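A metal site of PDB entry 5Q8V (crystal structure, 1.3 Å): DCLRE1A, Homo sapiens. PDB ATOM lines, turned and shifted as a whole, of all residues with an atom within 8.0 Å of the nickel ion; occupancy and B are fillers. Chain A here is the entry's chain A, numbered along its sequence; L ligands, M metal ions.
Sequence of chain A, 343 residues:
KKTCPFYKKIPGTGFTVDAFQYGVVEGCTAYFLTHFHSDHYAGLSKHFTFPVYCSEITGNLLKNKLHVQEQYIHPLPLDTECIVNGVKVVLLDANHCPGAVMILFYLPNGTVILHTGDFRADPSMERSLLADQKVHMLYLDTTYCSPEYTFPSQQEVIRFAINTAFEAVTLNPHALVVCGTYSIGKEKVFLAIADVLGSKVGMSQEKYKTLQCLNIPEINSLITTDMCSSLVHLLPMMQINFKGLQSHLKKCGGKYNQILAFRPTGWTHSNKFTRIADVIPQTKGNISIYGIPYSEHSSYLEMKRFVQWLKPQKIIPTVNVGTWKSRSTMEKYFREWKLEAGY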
ATOM      1  N   ASP A  18      18.256 -27.791  -0.934  1.00  0.00           N
ATOM      2  CA  ASP A  18      18.001 -26.545  -0.191  1.00  0.00           C
ATOM      3  C   ASP A  18      16.942 -25.636  -0.934  1.00  0.00           C
ATOM      4  O   ASP A  18      17.122 -24.393  -0.989  1.00  0.00           O
ATOM      5  CB  ASP A  18      19.295 -25.830   0.176  1.00  0.00           C
ATOM      6  CG  ASP A  18      20.248 -26.692   1.047  1.00  0.00           C
ATOM      7  OD1 ASP A  18      19.784 -27.740   1.569  1.00  0.00           O
ATOM      8  OD2 ASP A  18      21.432 -26.225   1.160  1.00  0.00           O
ATOM      9  N   THR A  34      20.855 -29.780   3.242  1.00  0.00           N
ATOM     10  CA  THR A  34      22.282 -29.904   3.630  1.00  0.00           C
ATOM     11  C   THR A  34      22.493 -29.653   5.151  1.00  0.00           C
ATOM     12  O   THR A  34      23.352 -30.314   5.764  1.00  0.00           O
ATOM     13  CB  THR A  34      23.260 -29.050   2.806  1.00  0.00           C
ATOM     14  OG1 THR A  34      22.919 -27.640   2.986  1.00  0.00           O
ATOM     15  CG2 THR A  34      23.210 -29.394   1.290  1.00  0.00           C
ATOM     16  N   HIS A  35      21.745 -28.685   5.736  1.00  0.00           N
ATOM     17  CA  HIS A  35      21.952 -28.257   7.113  1.00  0.00           C
ATOM     18  C   HIS A  35      20.798 -27.437   7.600  1.00  0.00           C
ATOM     19  O   HIS A  35      20.110 -26.782   6.777  1.00  0.00           O
ATOM     20  CB  HIS A  35      23.352 -27.603   7.349  1.00  0.00           C
ATOM     21  CG  HIS A  35      23.545 -26.273   6.692  1.00  0.00           C
ATOM     22  ND1 HIS A  35      23.595 -26.036   5.332  1.00  0.00           N
ATOM     23  CD2 HIS A  35      23.697 -25.067   7.268  1.00  0.00           C
ATOM     24  CE1 HIS A  35      23.806 -24.733   5.138  1.00  0.00           C
ATOM     25  NE2 HIS A  35      23.932 -24.163   6.288  1.00  0.00           N
ATOM     26  N   PHE A  36      20.702 -27.341   8.911  1.00  0.00           N
ATOM     27  CA  PHE A  36      19.585 -26.527   9.541  1.00  0.00           C
ATOM     28  C   PHE A  36      19.991 -25.085   9.789  1.00  0.00           C
ATOM     29  O   PHE A  36      20.111 -24.658  11.007  1.00  0.00           O
ATOM     30  CB  PHE A  36      19.168 -27.245  10.908  1.00  0.00           C
ATOM     31  CG  PHE A  36      17.824 -26.790  11.484  1.00  0.00           C
ATOM     32  CD1 PHE A  36      16.646 -27.272  10.927  1.00  0.00           C
ATOM     33  CD2 PHE A  36      17.799 -25.965  12.572  1.00  0.00           C
ATOM     34  CE1 PHE A  36      15.405 -26.869  11.449  1.00  0.00           C
ATOM     35  CE2 PHE A  36      16.568 -25.546  13.119  1.00  0.00           C
ATOM     36  CZ  PHE A  36      15.411 -26.004  12.587  1.00  0.00           C
ATOM     37  N   HIS A  37      20.149 -24.296   8.726  1.00  0.00           N
ATOM     38  CA  HIS A  37      20.266 -22.824   8.760  1.00  0.00           C
ATOM     39  C   HIS A  37      19.078 -22.258   7.978  1.00  0.00           C
ATOM     40  O   HIS A  37      18.680 -22.796   6.914  1.00  0.00           O
ATOM     41  CB  HIS A  37      21.617 -22.293   8.226  1.00  0.00           C
ATOM     42  CG  HIS A  37      22.764 -22.369   9.196  1.00  0.00           C
ATOM     43  ND1 HIS A  37      24.090 -22.229   8.832  1.00  0.00           N
ATOM     44  CD2 HIS A  37      22.765 -22.475  10.545  1.00  0.00           C
ATOM     45  CE1 HIS A  37      24.873 -22.266   9.897  1.00  0.00           C
ATOM     46  NE2 HIS A  37      24.098 -22.462  10.942  1.00  0.00           N
ATOM     47  N   SER A  38      18.504 -21.141   8.459  1.00  0.00           N
ATOM     48  CA  SER A  38      17.170 -20.648   7.947  1.00  0.00           C
ATOM     49  C   SER A  38      17.180 -20.327   6.452  1.00  0.00           C
ATOM     50  O   SER A  38      16.134 -20.643   5.829  1.00  0.00           O
ATOM     51  CB  SER A  38      16.592 -19.523   8.844  1.00  0.00           C
ATOM     52  OG  SER A  38      17.450 -18.431   8.836  1.00  0.00           O
ATOM     53  N   ASP A  39      18.264 -19.789   5.910  1.00  0.00           N
ATOM     54  CA  ASP A  39      18.288 -19.422   4.440  1.00  0.00           C
ATOM     55  C   ASP A  39      18.114 -20.707   3.627  1.00  0.00           C
ATOM     56  O   ASP A  39      17.746 -20.652   2.433  1.00  0.00           O
ATOM     57  CB  ASP A  39      19.547 -18.728   4.071  1.00  0.00           C
ATOM     58  CG  ASP A  39      19.546 -17.164   4.367  1.00  0.00           C
ATOM     59  OD1 ASP A  39      18.522 -16.678   4.848  1.00  0.00           O
ATOM     60  OD2 ASP A  39      20.613 -16.552   4.148  1.00  0.00           O
ATOM     61  N   HIS A  40      18.488 -21.877   4.213  1.00  0.00           N
ATOM     62  CA  HIS A  40      18.461 -23.177   3.521  1.00  0.00           C
ATOM     63  C   HIS A  40      17.228 -23.944   3.758  1.00  0.00           C
ATOM     64  O   HIS A  40      16.693 -24.576   2.793  1.00  0.00           O
ATOM     65  CB  HIS A  40      19.756 -24.020   3.906  1.00  0.00           C
ATOM     66  CG  HIS A  40      20.994 -23.330   3.493  1.00  0.00           C
ATOM     67  ND1 HIS A  40      21.744 -23.677   2.387  1.00  0.00           N
ATOM     68  CD2 HIS A  40      21.618 -22.246   4.018  1.00  0.00           C
ATOM     69  CE1 HIS A  40      22.767 -22.858   2.265  1.00  0.00           C
ATOM     70  NE2 HIS A  40      22.708 -21.972   3.254  1.00  0.00           N
ATOM     71  N   HIS A  96      30.940 -27.650   8.897  1.00  0.00           N
ATOM     72  CA  HIS A  96      30.129 -26.378   9.009  1.00  0.00           C
ATOM     73  C   HIS A  96      29.534 -26.421  10.411  1.00  0.00           C
ATOM     74  O   HIS A  96      30.380 -26.365  11.358  1.00  0.00           O
ATOM     75  CB  HIS A  96      29.199 -26.241   7.836  1.00  0.00           C
ATOM     76  CG  HIS A  96      28.390 -24.960   7.718  1.00  0.00           C
ATOM     77  ND1 HIS A  96      28.996 -23.737   7.765  1.00  0.00           N
ATOM     78  CD2 HIS A  96      27.065 -24.743   7.698  1.00  0.00           C
ATOM     79  CE1 HIS A  96      28.039 -22.808   7.668  1.00  0.00           C
ATOM     80  NE2 HIS A  96      26.853 -23.376   7.574  1.00  0.00           N
ATOM     81  N   CYS A  97      28.242 -26.401  10.564  1.00  0.00           N
ATOM     82  CA  CYS A  97      27.569 -26.526  11.868  1.00  0.00           C
ATOM     83  C   CYS A  97      27.197 -28.011  12.154  1.00  0.00           C
ATOM     84  O   CYS A  97      27.302 -28.848  11.242  1.00  0.00           O
ATOM     85  CB  CYS A  97      26.319 -25.609  11.854  1.00  0.00           C
ATOM     86  SG  CYS A  97      25.047 -26.135  10.637  1.00  0.00           S
ATOM     87  N   ALA A 100      25.643 -30.714   9.420  1.00  0.00           N
ATOM     88  CA  ALA A 100      25.871 -30.233   8.041  1.00  0.00           C
ATOM     89  C   ALA A 100      26.597 -31.225   7.182  1.00  0.00           C
ATOM     90  O   ALA A 100      27.646 -31.757   7.631  1.00  0.00           O
ATOM     91  CB  ALA A 100      26.582 -28.897   8.048  1.00  0.00           C
ATOM     92  N   GLY A 117      27.037 -28.007  -0.053  1.00  0.00           N
ATOM     93  CA  GLY A 117      26.264 -27.262   0.899  1.00  0.00           C
ATOM     94  C   GLY A 117      27.077 -26.079   1.342  1.00  0.00           C
ATOM     95  O   GLY A 117      27.807 -25.485   0.582  1.00  0.00           O
ATOM     96  N   ASP A 118      26.913 -25.672   2.595  1.00  0.00           N
ATOM     97  CA  ASP A 118      27.872 -24.761   3.272  1.00  0.00           C
ATOM     98  C   ASP A 118      29.013 -25.592   3.881  1.00  0.00           C
ATOM     99  O   ASP A 118      28.757 -26.630   4.529  1.00  0.00           O
ATOM    100  CB  ASP A 118      27.198 -23.920   4.358  1.00  0.00           C
ATOM    101  CG  ASP A 118      26.359 -22.752   3.829  1.00  0.00           C
ATOM    102  OD1 ASP A 118      26.417 -22.362   2.641  1.00  0.00           O
ATOM    103  OD2 ASP A 118      25.751 -22.108   4.708  1.00  0.00           O
ATOM    104  N   PHE A 119      30.234 -25.166   3.684  1.00  0.00           N
ATOM    105  CA  PHE A 119      31.411 -25.947   4.193  1.00  0.00           C
ATOM    106  C   PHE A 119      32.603 -25.102   4.601  1.00  0.00           C
ATOM    107  O   PHE A 119      32.757 -23.991   4.066  1.00  0.00           O
ATOM    108  CB  PHE A 119      31.816 -27.155   3.265  1.00  0.00           C
ATOM    109  CG  PHE A 119      32.782 -26.874   2.082  1.00  0.00           C
ATOM    110  CD1 PHE A 119      33.773 -27.771   1.732  1.00  0.00           C
ATOM    111  CD2 PHE A 119      32.711 -25.696   1.290  1.00  0.00           C
ATOM    112  CE1 PHE A 119      34.596 -27.576   0.645  1.00  0.00           C
ATOM    113  CE2 PHE A 119      33.573 -25.479   0.214  1.00  0.00           C
ATOM    114  CZ  PHE A 119      34.502 -26.431  -0.109  1.00  0.00           C
ATOM    115  N   ASP A 141      30.230 -23.746  -2.260  1.00  0.00           N
ATOM    116  CA  ASP A 141      30.013 -22.630  -1.267  1.00  0.00           C
ATOM    117  C   ASP A 141      31.170 -21.673  -1.464  1.00  0.00           C
ATOM    118  O   ASP A 141      32.309 -21.854  -1.017  1.00  0.00           O
ATOM    119  CB  ASP A 141      30.013 -23.179   0.150  1.00  0.00           C
ATOM    120  CG  ASP A 141      30.090 -22.093   1.217  1.00  0.00           C
ATOM    121  OD1 ASP A 141      29.879 -20.891   0.859  1.00  0.00           O
ATOM    122  OD2 ASP A 141      30.350 -22.456   2.386  1.00  0.00           O
ATOM    123  N   THR A 143      31.110 -18.389  -0.397  1.00  0.00           N
ATOM    124  CA  THR A 143      30.949 -17.279   0.519  1.00  0.00           C
ATOM    125  C   THR A 143      32.108 -16.331   0.581  1.00  0.00           C
ATOM    126  O   THR A 143      31.940 -15.092   0.399  1.00  0.00           O
ATOM    127  CB  THR A 143      30.576 -17.803   1.968  1.00  0.00           C
ATOM    128  OG1 THR A 143      29.339 -18.524   1.943  1.00  0.00           O
ATOM    129  CG2 THR A 143      30.409 -16.666   2.980  1.00  0.00           C
ATOM    130  N   SER A 183      21.721 -18.969  15.716  1.00  0.00           N
ATOM    131  CA  SER A 183      21.542 -20.156  14.891  1.00  0.00           C
ATOM    132  C   SER A 183      22.402 -21.257  15.536  1.00  0.00           C
ATOM    133  O   SER A 183      23.278 -20.974  16.408  1.00  0.00           O
ATOM    134  CB  SER A 183      22.076 -19.937  13.445  1.00  0.00           C
ATOM    135  OG  SER A 183      23.482 -19.636  13.468  1.00  0.00           O
ATOM    136  N   ILE A 184      22.273 -22.478  15.103  1.00  0.00           N
ATOM    137  CA  ILE A 184      23.236 -23.487  15.479  1.00  0.00           C
ATOM    138  C   ILE A 184      24.561 -23.215  14.779  1.00  0.00           C
ATOM    139  O   ILE A 184      24.646 -22.421  13.792  1.00  0.00           O
ATOM    140  CB  ILE A 184      22.770 -24.936  15.156  1.00  0.00           C
ATOM    141  CG1 ILE A 184      22.624 -25.232  13.659  1.00  0.00           C
ATOM    142  CG2 ILE A 184      21.504 -25.283  15.931  1.00  0.00           C
ATOM    143  CD1 ILE A 184      22.450 -26.702  13.270  1.00  0.00           C
ATOM    144  N   GLU A 296      32.841 -20.687  10.153  1.00  0.00           N
ATOM    145  CA  GLU A 296      32.438 -22.039   9.675  1.00  0.00           C
ATOM    146  C   GLU A 296      32.283 -22.147   8.127  1.00  0.00           C
ATOM    147  O   GLU A 296      31.644 -23.060   7.591  1.00  0.00           O
ATOM    148  CB  GLU A 296      31.189 -22.544  10.413  1.00  0.00           C
ATOM    149  CG  GLU A 296      31.525 -22.886  11.960  1.00  0.00           C
ATOM    150  CD  GLU A 296      30.403 -23.535  12.751  1.00  0.00           C
ATOM    151  OE1 GLU A 296      29.196 -23.418  12.361  1.00  0.00           O
ATOM    152  OE2 GLU A 296      30.725 -24.124  13.844  1.00  0.00           O
ATOM    153  N   HIS A 297      32.901 -21.153   7.458  1.00  0.00           N
ATOM    154  CA  HIS A 297      33.094 -21.250   6.013  1.00  0.00           C
ATOM    155  C   HIS A 297      34.595 -21.219   5.608  1.00  0.00           C
ATOM    156  O   HIS A 297      35.437 -20.647   6.350  1.00  0.00           O
ATOM    157  CB  HIS A 297      32.402 -20.063   5.252  1.00  0.00           C
ATOM    158  CG  HIS A 297      30.912 -19.999   5.382  1.00  0.00           C
ATOM    159  ND1 HIS A 297      30.051 -20.674   4.528  1.00  0.00           N
ATOM    160  CD2 HIS A 297      30.098 -19.290   6.240  1.00  0.00           C
ATOM    161  CE1 HIS A 297      28.797 -20.431   4.872  1.00  0.00           C
ATOM    162  NE2 HIS A 297      28.832 -19.601   5.904  1.00  0.00           N
HETATM  163  C1  LIG L   1      24.345 -18.983   7.316  1.00  0.00           C
HETATM  164  C2  LIG L   1      25.840 -19.276   7.248  1.00  0.00           C
HETATM  165  C3  LIG L   1      23.543 -19.711   6.230  1.00  0.00           C
HETATM  166  O1  LIG L   1      26.686 -18.387   7.258  1.00  0.00           O
HETATM  167  O2  LIG L   1      26.127 -20.424   7.199  1.00  0.00           O
HETATM  168  O3  LIG L   1      23.641 -20.929   6.066  1.00  0.00           O
HETATM  169  O4  LIG L   1      22.673 -19.042   5.585  1.00  0.00           O
HETATM  170 NI    NI M   1      25.013 -22.228   6.784  1.00  0.00          NI
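OD2 of Asp 118 sits close to NE2 of His 40 (3.4 Å). A ring nitrogen (NE2) of His 37 lies within hydrogen-bond range of the backbone carbonyl oxygen (O) of Ile 184. The side-chain hydroxyl (OG1) of Thr 34 lies within hydrogen-bond range of a ring nitrogen (ND1) of His 35. ND1 of His 96 is in hydrogen-bond range of O of Glu 296, at 2.7 Å.
An oxygen (O3) of the ligand is bound to the nickel ion (2.0 Å). O2 of the ligand is bound to the nickel ion (2.2 Å). The side-chain carboxylate (OD2) of Asp 118 is bound to the nickel ion (2.2 Å). ND1 of His 37 is bound to the nickel ion, 2.2 Å away. The nickel ion is bound by NE2 of His 35 (2.3 Å). NE2 of His 96 is bound to the nickel ion (2.3 Å). The nickel ion has six donor atoms within binding distance.
Of the 20 residues printed, 4 come within 4 Å of the nickel ion. Along chain A the residues within 4 Å of the nickel ion span positions 35 to 118. The nearest printed residue that does not touch the nickel ion is His 40 (4.2 Å).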
